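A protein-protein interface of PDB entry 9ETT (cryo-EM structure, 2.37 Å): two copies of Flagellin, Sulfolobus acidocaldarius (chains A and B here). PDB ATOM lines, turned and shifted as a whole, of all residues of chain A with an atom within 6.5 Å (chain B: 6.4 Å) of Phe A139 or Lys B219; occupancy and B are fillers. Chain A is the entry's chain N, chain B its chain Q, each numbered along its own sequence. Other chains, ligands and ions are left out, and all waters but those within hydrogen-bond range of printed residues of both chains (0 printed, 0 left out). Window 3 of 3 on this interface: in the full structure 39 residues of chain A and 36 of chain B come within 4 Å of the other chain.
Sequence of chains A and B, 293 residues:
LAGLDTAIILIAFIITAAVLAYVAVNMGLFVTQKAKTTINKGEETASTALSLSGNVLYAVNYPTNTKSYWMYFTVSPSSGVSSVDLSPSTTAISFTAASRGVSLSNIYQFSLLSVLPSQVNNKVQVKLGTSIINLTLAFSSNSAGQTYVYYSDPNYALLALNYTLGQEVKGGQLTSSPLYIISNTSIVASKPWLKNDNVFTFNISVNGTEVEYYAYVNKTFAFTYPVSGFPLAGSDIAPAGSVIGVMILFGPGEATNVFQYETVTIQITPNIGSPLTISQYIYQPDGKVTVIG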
ATOM      1  N   PRO A 117      28.017  -7.441 -22.224  1.00  0.00           N
ATOM      2  CA  PRO A 117      27.239  -8.575 -21.720  1.00  0.00           C
ATOM      3  C   PRO A 117      27.690  -9.935 -22.255  1.00  0.00           C
ATOM      4  O   PRO A 117      27.758 -10.886 -21.482  1.00  0.00           O
ATOM      5  CB  PRO A 117      25.798  -8.265 -22.147  1.00  0.00           C
ATOM      6  CG  PRO A 117      25.771  -6.764 -22.261  1.00  0.00           C
ATOM      7  CD  PRO A 117      27.149  -6.386 -22.763  1.00  0.00           C
ATOM      8  N   ASN A 121      27.707 -13.139 -19.740  1.00  0.00           N
ATOM      9  CA  ASN A 121      26.518 -13.978 -19.838  1.00  0.00           C
ATOM     10  C   ASN A 121      26.865 -15.340 -20.444  1.00  0.00           C
ATOM     11  O   ASN A 121      27.673 -15.415 -21.365  1.00  0.00           O
ATOM     12  CB  ASN A 121      25.423 -13.249 -20.618  1.00  0.00           C
ATOM     13  CG  ASN A 121      24.864 -12.055 -19.871  1.00  0.00           C
ATOM     14  OD1 ASN A 121      25.045 -11.926 -18.665  1.00  0.00           O
ATOM     15  ND2 ASN A 121      24.158 -11.175 -20.559  1.00  0.00           N
ATOM     16  N   THR A 136      22.726 -15.673 -16.523  1.00  0.00           N
ATOM     17  CA  THR A 136      22.701 -14.340 -17.110  1.00  0.00           C
ATOM     18  C   THR A 136      22.947 -13.341 -15.985  1.00  0.00           C
ATOM     19  O   THR A 136      22.225 -13.347 -14.991  1.00  0.00           O
ATOM     20  CB  THR A 136      21.363 -14.046 -17.806  1.00  0.00           C
ATOM     21  OG1 THR A 136      21.153 -15.005 -18.842  1.00  0.00           O
ATOM     22  CG2 THR A 136      21.281 -12.656 -18.402  1.00  0.00           C
ATOM     23  N   LEU A 137      23.978 -12.496 -16.142  1.00  0.00           N
ATOM     24  CA  LEU A 137      24.465 -11.627 -15.076  1.00  0.00           C
ATOM     25  C   LEU A 137      24.309 -10.155 -15.452  1.00  0.00           C
ATOM     26  O   LEU A 137      23.778  -9.381 -14.665  1.00  0.00           O
ATOM     27  CB  LEU A 137      25.915 -11.988 -14.738  1.00  0.00           C
ATOM     28  CG  LEU A 137      26.123 -13.460 -14.387  1.00  0.00           C
ATOM     29  CD1 LEU A 137      26.752 -14.206 -15.546  1.00  0.00           C
ATOM     30  CD2 LEU A 137      27.003 -13.617 -13.169  1.00  0.00           C
ATOM     31  N   ALA A 138      24.739  -9.787 -16.664  1.00  0.00           N
ATOM     32  CA  ALA A 138      24.485  -8.472 -17.228  1.00  0.00           C
ATOM     33  C   ALA A 138      23.108  -8.471 -17.895  1.00  0.00           C
ATOM     34  O   ALA A 138      22.906  -9.132 -18.909  1.00  0.00           O
ATOM     35  CB  ALA A 138      25.590  -8.138 -18.204  1.00  0.00           C
ATOM     36  N   PHE A 139      22.155  -7.732 -17.320  1.00  0.00           N
ATOM     37  CA  PHE A 139      20.864  -7.509 -17.953  1.00  0.00           C
ATOM     38  C   PHE A 139      20.989  -6.365 -18.959  1.00  0.00           C
ATOM     39  O   PHE A 139      21.906  -5.550 -18.875  1.00  0.00           O
ATOM     40  CB  PHE A 139      19.785  -7.227 -16.903  1.00  0.00           C
ATOM     41  CG  PHE A 139      19.451  -8.334 -15.921  1.00  0.00           C
ATOM     42  CD1 PHE A 139      20.013  -9.606 -16.011  1.00  0.00           C
ATOM     43  CD2 PHE A 139      18.527  -8.109 -14.906  1.00  0.00           C
ATOM     44  CE1 PHE A 139      19.695 -10.602 -15.094  1.00  0.00           C
ATOM     45  CE2 PHE A 139      18.197  -9.106 -13.996  1.00  0.00           C
ATOM     46  CZ  PHE A 139      18.790 -10.347 -14.083  1.00  0.00           C
ATOM     47  N   SER A 140      20.057  -6.304 -19.918  1.00  0.00           N
ATOM     48  CA  SER A 140      20.118  -5.300 -20.973  1.00  0.00           C
ATOM     49  C   SER A 140      18.726  -4.946 -21.503  1.00  0.00           C
ATOM     50  O   SER A 140      17.817  -5.774 -21.465  1.00  0.00           O
ATOM     51  CB  SER A 140      21.051  -5.758 -22.066  1.00  0.00           C
ATOM     52  OG  SER A 140      21.191  -4.767 -23.068  1.00  0.00           O
ATOM     53  N   SER A 141      18.571  -3.704 -21.998  1.00  0.00           N
ATOM     54  CA  SER A 141      17.345  -3.213 -22.619  1.00  0.00           C
ATOM     55  C   SER A 141      17.675  -2.164 -23.686  1.00  0.00           C
ATOM     56  O   SER A 141      18.763  -1.596 -23.682  1.00  0.00           O
ATOM     57  CB  SER A 141      16.378  -2.682 -21.587  1.00  0.00           C
ATOM     58  OG  SER A 141      16.923  -1.571 -20.891  1.00  0.00           O
ATOM     59  N   TYR A 148      21.315  -0.470 -23.355  1.00  0.00           N
ATOM     60  CA  TYR A 148      21.674  -0.172 -21.976  1.00  0.00           C
ATOM     61  C   TYR A 148      22.090  -1.474 -21.295  1.00  0.00           C
ATOM     62  O   TYR A 148      21.553  -2.532 -21.607  1.00  0.00           O
ATOM     63  CB  TYR A 148      20.505   0.548 -21.294  1.00  0.00           C
ATOM     64  CG  TYR A 148      20.310   1.941 -21.841  1.00  0.00           C
ATOM     65  CD1 TYR A 148      19.739   2.143 -23.092  1.00  0.00           C
ATOM     66  CD2 TYR A 148      20.749   3.061 -21.143  1.00  0.00           C
ATOM     67  CE1 TYR A 148      19.614   3.414 -23.630  1.00  0.00           C
ATOM     68  CE2 TYR A 148      20.635   4.343 -21.666  1.00  0.00           C
ATOM     69  CZ  TYR A 148      20.070   4.519 -22.925  1.00  0.00           C
ATOM     70  OH  TYR A 148      19.930   5.760 -23.493  1.00  0.00           O
ATOM     71  N   VAL A 149      23.067  -1.401 -20.383  1.00  0.00           N
ATOM     72  CA  VAL A 149      23.594  -2.576 -19.699  1.00  0.00           C
ATOM     73  C   VAL A 149      23.637  -2.281 -18.203  1.00  0.00           C
ATOM     74  O   VAL A 149      24.024  -1.185 -17.805  1.00  0.00           O
ATOM     75  CB  VAL A 149      24.996  -2.954 -20.226  1.00  0.00           C
ATOM     76  CG1 VAL A 149      25.643  -4.072 -19.419  1.00  0.00           C
ATOM     77  CG2 VAL A 149      24.952  -3.322 -21.699  1.00  0.00           C
ATOM     78  N   TYR A 150      23.260  -3.266 -17.378  1.00  0.00           N
ATOM     79  CA  TYR A 150      23.359  -3.105 -15.934  1.00  0.00           C
ATOM     80  C   TYR A 150      23.398  -4.460 -15.234  1.00  0.00           C
ATOM     81  O   TYR A 150      23.028  -5.478 -15.809  1.00  0.00           O
ATOM     82  CB  TYR A 150      22.197  -2.261 -15.398  1.00  0.00           C
ATOM     83  CG  TYR A 150      20.839  -2.913 -15.477  1.00  0.00           C
ATOM     84  CD1 TYR A 150      20.093  -2.876 -16.649  1.00  0.00           C
ATOM     85  CD2 TYR A 150      20.306  -3.577 -14.380  1.00  0.00           C
ATOM     86  CE1 TYR A 150      18.850  -3.483 -16.726  1.00  0.00           C
ATOM     87  CE2 TYR A 150      19.062  -4.186 -14.443  1.00  0.00           C
ATOM     88  CZ  TYR A 150      18.334  -4.142 -15.620  1.00  0.00           C
ATOM     89  OH  TYR A 150      17.109  -4.746 -15.680  1.00  0.00           O
ATOM     90  N   TYR A 151      23.817  -4.450 -13.964  1.00  0.00           N
ATOM     91  CA  TYR A 151      23.748  -5.617 -13.098  1.00  0.00           C
ATOM     92  C   TYR A 151      22.667  -5.357 -12.054  1.00  0.00           C
ATOM     93  O   TYR A 151      22.660  -4.316 -11.400  1.00  0.00           O
ATOM     94  CB  TYR A 151      25.128  -5.929 -12.512  1.00  0.00           C
ATOM     95  CG  TYR A 151      26.174  -6.199 -13.564  1.00  0.00           C
ATOM     96  CD1 TYR A 151      26.773  -5.151 -14.259  1.00  0.00           C
ATOM     97  CD2 TYR A 151      26.526  -7.501 -13.903  1.00  0.00           C
ATOM     98  CE1 TYR A 151      27.680  -5.388 -15.282  1.00  0.00           C
ATOM     99  CE2 TYR A 151      27.448  -7.747 -14.912  1.00  0.00           C
ATOM    100  CZ  TYR A 151      28.027  -6.691 -15.600  1.00  0.00           C
ATOM    101  OH  TYR A 151      28.932  -6.943 -16.595  1.00  0.00           O
ATOM    102  N   SER A 152      21.741  -6.308 -11.912  1.00  0.00           N
ATOM    103  CA  SER A 152      20.565  -6.111 -11.075  1.00  0.00           C
ATOM    104  C   SER A 152      20.917  -6.064  -9.586  1.00  0.00           C
ATOM    105  O   SER A 152      20.194  -5.438  -8.813  1.00  0.00           O
ATOM    106  CB  SER A 152      19.515  -7.146 -11.354  1.00  0.00           C
ATOM    107  OG  SER A 152      20.025  -8.448 -11.128  1.00  0.00           O
ATOM    108  N   TYR A 156      25.360 -10.638  -8.759  1.00  0.00           N
ATOM    109  CA  TYR A 156      25.641 -10.870 -10.169  1.00  0.00           C
ATOM    110  C   TYR A 156      26.838 -10.047 -10.644  1.00  0.00           C
ATOM    111  O   TYR A 156      27.615 -10.521 -11.462  1.00  0.00           O
ATOM    112  CB  TYR A 156      24.392 -10.627 -11.013  1.00  0.00           C
ATOM    113  CG  TYR A 156      23.269 -11.599 -10.748  1.00  0.00           C
ATOM    114  CD1 TYR A 156      23.453 -12.971 -10.864  1.00  0.00           C
ATOM    115  CD2 TYR A 156      22.008 -11.148 -10.383  1.00  0.00           C
ATOM    116  CE1 TYR A 156      22.419 -13.867 -10.619  1.00  0.00           C
ATOM    117  CE2 TYR A 156      20.961 -12.029 -10.141  1.00  0.00           C
ATOM    118  CZ  TYR A 156      21.168 -13.393 -10.258  1.00  0.00           C
ATOM    119  OH  TYR A 156      20.141 -14.267 -10.018  1.00  0.00           O
ATOM    120  N   SER A 205      19.617 -17.462  -6.559  1.00  0.00           N
ATOM    121  CA  SER A 205      18.682 -18.543  -6.863  1.00  0.00           C
ATOM    122  C   SER A 205      18.795 -18.981  -8.327  1.00  0.00           C
ATOM    123  O   SER A 205      18.776 -18.150  -9.233  1.00  0.00           O
ATOM    124  CB  SER A 205      17.255 -18.218  -6.455  1.00  0.00           C
ATOM    125  OG  SER A 205      16.706 -17.157  -7.226  1.00  0.00           O
ATOM    126  N   ASN B 106      19.282  -2.690  -9.002  1.00  0.00           N
ATOM    127  CA  ASN B 106      18.270  -2.275  -9.963  1.00  0.00           C
ATOM    128  C   ASN B 106      17.374  -3.444 -10.369  1.00  0.00           C
ATOM    129  O   ASN B 106      17.830  -4.382 -11.014  1.00  0.00           O
ATOM    130  CB  ASN B 106      18.887  -1.607 -11.193  1.00  0.00           C
ATOM    131  CG  ASN B 106      17.845  -0.995 -12.100  1.00  0.00           C
ATOM    132  OD1 ASN B 106      16.678  -0.866 -11.728  1.00  0.00           O
ATOM    133  ND2 ASN B 106      18.265  -0.581 -13.280  1.00  0.00           N
ATOM    134  N   GLN B 109      12.462  -3.030 -14.846  1.00  0.00           N
ATOM    135  CA  GLN B 109      12.662  -3.639 -16.157  1.00  0.00           C
ATOM    136  C   GLN B 109      11.697  -3.126 -17.230  1.00  0.00           C
ATOM    137  O   GLN B 109      12.097  -2.983 -18.384  1.00  0.00           O
ATOM    138  CB  GLN B 109      12.633  -5.163 -16.053  1.00  0.00           C
ATOM    139  CG  GLN B 109      13.773  -5.702 -15.203  1.00  0.00           C
ATOM    140  CD  GLN B 109      14.060  -7.172 -15.378  1.00  0.00           C
ATOM    141  OE1 GLN B 109      13.869  -7.746 -16.448  1.00  0.00           O
ATOM    142  NE2 GLN B 109      14.567  -7.794 -14.325  1.00  0.00           N
ATOM    143  N   SER B 176      13.875 -13.526 -22.800  1.00  0.00           N
ATOM    144  CA  SER B 176      12.812 -14.219 -22.080  1.00  0.00           C
ATOM    145  C   SER B 176      11.998 -13.214 -21.268  1.00  0.00           C
ATOM    146  O   SER B 176      12.563 -12.296 -20.680  1.00  0.00           O
ATOM    147  CB  SER B 176      13.378 -15.266 -21.147  1.00  0.00           C
ATOM    148  OG  SER B 176      13.900 -16.374 -21.861  1.00  0.00           O
ATOM    149  N   SER B 177      10.680 -13.440 -21.165  1.00  0.00           N
ATOM    150  CA  SER B 177       9.860 -12.718 -20.205  1.00  0.00           C
ATOM    151  C   SER B 177      10.104 -13.300 -18.815  1.00  0.00           C
ATOM    152  O   SER B 177      10.027 -14.512 -18.650  1.00  0.00           O
ATOM    153  CB  SER B 177       8.398 -12.789 -20.558  1.00  0.00           C
ATOM    154  OG  SER B 177       7.630 -12.118 -19.573  1.00  0.00           O
ATOM    155  N   PRO B 178      10.358 -12.482 -17.766  1.00  0.00           N
ATOM    156  CA  PRO B 178      10.438 -12.993 -16.400  1.00  0.00           C
ATOM    157  C   PRO B 178       9.061 -13.291 -15.805  1.00  0.00           C
ATOM    158  O   PRO B 178       8.986 -13.915 -14.762  1.00  0.00           O
ATOM    159  CB  PRO B 178      11.135 -11.857 -15.636  1.00  0.00           C
ATOM    160  CG  PRO B 178      10.695 -10.614 -16.369  1.00  0.00           C
ATOM    161  CD  PRO B 178      10.589 -11.032 -17.822  1.00  0.00           C
ATOM    162  N   ASP B 197      10.202 -21.602  -9.956  1.00  0.00           N
ATOM    163  CA  ASP B 197      10.107 -20.149  -9.791  1.00  0.00           C
ATOM    164  C   ASP B 197       8.862 -19.732  -8.985  1.00  0.00           C
ATOM    165  O   ASP B 197       8.004 -20.558  -8.667  1.00  0.00           O
ATOM    166  CB  ASP B 197      10.391 -19.408 -11.106  1.00  0.00           C
ATOM    167  CG  ASP B 197       9.276 -19.417 -12.145  1.00  0.00           C
ATOM    168  OD1 ASP B 197       8.154 -19.822 -11.804  1.00  0.00           O
ATOM    169  OD2 ASP B 197       9.544 -19.008 -13.299  1.00  0.00           O
ATOM    170  N   VAL B 217       6.864 -16.021 -11.774  1.00  0.00           N
ATOM    171  CA  VAL B 217       7.847 -14.946 -11.733  1.00  0.00           C
ATOM    172  C   VAL B 217       9.256 -15.522 -11.564  1.00  0.00           C
ATOM    173  O   VAL B 217       9.600 -16.099 -10.536  1.00  0.00           O
ATOM    174  CB  VAL B 217       7.496 -13.910 -10.644  1.00  0.00           C
ATOM    175  CG1 VAL B 217       8.532 -12.805 -10.564  1.00  0.00           C
ATOM    176  CG2 VAL B 217       6.131 -13.283 -10.867  1.00  0.00           C
ATOM    177  N   ASN B 218      10.086 -15.294 -12.579  1.00  0.00           N
ATOM    178  CA  ASN B 218      11.405 -15.878 -12.794  1.00  0.00           C
ATOM    179  C   ASN B 218      12.461 -15.277 -11.843  1.00  0.00           C
ATOM    180  O   ASN B 218      13.380 -15.966 -11.381  1.00  0.00           O
ATOM    181  CB  ASN B 218      11.766 -15.576 -14.251  1.00  0.00           C
ATOM    182  CG  ASN B 218      12.190 -16.766 -15.088  1.00  0.00           C
ATOM    183  OD1 ASN B 218      11.996 -17.925 -14.720  1.00  0.00           O
ATOM    184  ND2 ASN B 218      12.763 -16.501 -16.246  1.00  0.00           N
ATOM    185  N   LYS B 219      12.343 -13.966 -11.570  1.00  0.00           N
ATOM    186  CA  LYS B 219      13.305 -13.162 -10.816  1.00  0.00           C
ATOM    187  C   LYS B 219      12.585 -11.952 -10.216  1.00  0.00           C
ATOM    188  O   LYS B 219      11.538 -11.569 -10.724  1.00  0.00           O
ATOM    189  CB  LYS B 219      14.415 -12.667 -11.752  1.00  0.00           C
ATOM    190  CG  LYS B 219      13.952 -11.807 -12.925  1.00  0.00           C
ATOM    191  CD  LYS B 219      14.997 -11.603 -14.008  1.00  0.00           C
ATOM    192  CE  LYS B 219      15.109 -12.754 -14.987  1.00  0.00           C
ATOM    193  NZ  LYS B 219      16.241 -12.568 -15.928  1.00  0.00           N
ATOM    194  N   THR B 220      13.138 -11.330  -9.161  1.00  0.00           N
ATOM    195  CA  THR B 220      12.514 -10.125  -8.624  1.00  0.00           C
ATOM    196  C   THR B 220      12.653  -8.977  -9.623  1.00  0.00           C
ATOM    197  O   THR B 220      13.763  -8.640 -10.023  1.00  0.00           O
ATOM    198  CB  THR B 220      13.090  -9.700  -7.266  1.00  0.00           C
ATOM    199  OG1 THR B 220      12.780 -10.745  -6.350  1.00  0.00           O
ATOM    200  CG2 THR B 220      12.470  -8.431  -6.721  1.00  0.00           C
ATOM    201  N   PHE B 221      11.520  -8.375 -10.015  1.00  0.00           N
ATOM    202  CA  PHE B 221      11.525  -7.254 -10.946  1.00  0.00           C
ATOM    203  C   PHE B 221      10.421  -6.258 -10.598  1.00  0.00           C
ATOM    204  O   PHE B 221       9.445  -6.602  -9.940  1.00  0.00           O
ATOM    205  CB  PHE B 221      11.459  -7.731 -12.403  1.00  0.00           C
ATOM    206  CG  PHE B 221      10.083  -8.082 -12.911  1.00  0.00           C
ATOM    207  CD1 PHE B 221       9.263  -7.111 -13.481  1.00  0.00           C
ATOM    208  CD2 PHE B 221       9.613  -9.386 -12.832  1.00  0.00           C
ATOM    209  CE1 PHE B 221       7.994  -7.441 -13.940  1.00  0.00           C
ATOM    210  CE2 PHE B 221       8.346  -9.715 -13.293  1.00  0.00           C
ATOM    211  CZ  PHE B 221       7.541  -8.741 -13.844  1.00  0.00           C
ATOM    212  N   LEU B 249       7.319  -7.536  -8.261  1.00  0.00           N
ATOM    213  CA  LEU B 249       6.975  -8.947  -8.126  1.00  0.00           C
ATOM    214  C   LEU B 249       8.223  -9.695  -7.673  1.00  0.00           C
ATOM    215  O   LEU B 249       9.270  -9.555  -8.289  1.00  0.00           O
ATOM    216  CB  LEU B 249       6.484  -9.512  -9.465  1.00  0.00           C
ATOM    217  CG  LEU B 249       5.445  -8.702 -10.239  1.00  0.00           C
ATOM    218  CD1 LEU B 249       5.013  -9.485 -11.459  1.00  0.00           C
ATOM    219  CD2 LEU B 249       4.228  -8.381  -9.383  1.00  0.00           C
ATOM    220  N   PHE B 250       8.121 -10.486  -6.602  1.00  0.00           N
ATOM    221  CA  PHE B 250       9.286 -11.187  -6.074  1.00  0.00           C
ATOM    222  C   PHE B 250       9.553 -12.484  -6.834  1.00  0.00           C
ATOM    223  O   PHE B 250       8.631 -13.250  -7.109  1.00  0.00           O
ATOM    224  CB  PHE B 250       9.141 -11.410  -4.567  1.00  0.00           C
ATOM    225  CG  PHE B 250       9.046 -10.110  -3.812  1.00  0.00           C
ATOM    226  CD1 PHE B 250      10.139  -9.250  -3.749  1.00  0.00           C
ATOM    227  CD2 PHE B 250       7.848  -9.715  -3.224  1.00  0.00           C
ATOM    228  CE1 PHE B 250      10.041  -8.034  -3.087  1.00  0.00           C
ATOM    229  CE2 PHE B 250       7.749  -8.492  -2.573  1.00  0.00           C
ATOM    230  CZ  PHE B 250       8.850  -7.660  -2.502  1.00  0.00           C
ATOM    231  N   GLY B 251      10.835 -12.743  -7.128  1.00  0.00           N
ATOM    232  CA  GLY B 251      11.284 -14.015  -7.676  1.00  0.00           C
ATOM    233  C   GLY B 251      11.562 -15.042  -6.580  1.00  0.00           C
ATOM    234  O   GLY B 251      11.462 -14.732  -5.399  1.00  0.00           O
ATOM    235  N   PRO B 252      11.953 -16.288  -6.925  1.00  0.00           N
ATOM    236  CA  PRO B 252      12.117 -17.358  -5.944  1.00  0.00           C
ATOM    237  C   PRO B 252      13.207 -17.110  -4.901  1.00  0.00           C
ATOM    238  O   PRO B 252      13.121 -17.665  -3.814  1.00  0.00           O
ATOM    239  CB  PRO B 252      12.404 -18.604  -6.798  1.00  0.00           C
ATOM    240  CG  PRO B 252      12.983 -18.053  -8.078  1.00  0.00           C
ATOM    241  CD  PRO B 252      12.245 -16.751  -8.281  1.00  0.00           C
ATOM    242  N   GLU B 254      14.064 -13.758  -3.417  1.00  0.00           N
ATOM    243  CA  GLU B 254      13.526 -12.845  -2.410  1.00  0.00           C
ATOM    244  C   GLU B 254      12.193 -13.317  -1.822  1.00  0.00           C
ATOM    245  O   GLU B 254      11.837 -12.919  -0.714  1.00  0.00           O
ATOM    246  CB  GLU B 254      13.428 -11.418  -2.951  1.00  0.00           C
ATOM    247  CG  GLU B 254      14.791 -10.797  -3.230  1.00  0.00           C
ATOM    248  CD  GLU B 254      15.577 -11.427  -4.377  1.00  0.00           C
ATOM    249  OE1 GLU B 254      14.963 -11.731  -5.427  1.00  0.00           O
ATOM    250  OE2 GLU B 254      16.793 -11.659  -4.206  1.00  0.00           O
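Among the printed residues, merely in contact across the chains: Phe A139 with Gln B109 (3.9 Å), Phe A139 with Lys B219 (3.9 Å), Tyr A150 with Asn B106 (3.6 Å), Tyr A150 with Gln B109 (3.5 Å) and Ser A205 with Pro B252 (3.9 Å).
Of chain B, only Gln B109 and Lys B219 come within 4 Å of Phe A139. Printed residues of chain B within 4 Å of Ser A152: Asn B106 (2.9 Å). Of the printed residues of chain A, Asn B106 touches Tyr A150 (3.6 Å) and Ser A152 (2.9 Å). Printed residues of chain A within 4 Å of Pro B252: Ser A205. Pro A117 touches none of the printed residues of chain B. The nearest printed residue of chain B that does not touch Ser A205 is Asn B218 (5.5 Å).
No position is printed for both chains. Of the 6 pairs that touch across the chains among the printed residues, none has its exchanged pair printed and touching as well.
Printed residues of chain A that touch a printed residue of chain B: Phe A139, Tyr A150, Ser A152 and Ser A205. Of the 16 printed residues of chain B, 4 touch a printed residue of chain A. Printed residues of chain B that touch a printed residue of chain A: Asn B106, Gln B109, Lys B219 and Pro B252. Among the printed residues, no Asp or Glu carboxylate lies within 4 Å of a Lys or Arg side-chain nitrogen of the other chain.
The backbone carbonyl oxygen (O) of Ser A152 sits at hydrogen-bond distance from the backbone NH (N) of Asn B106 (2.9 Å).
The backbone carbonyl oxygen of Tyr A150 is in hydrogen-bond range of the backbone NH of Phe A139, 2.9 Å away.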
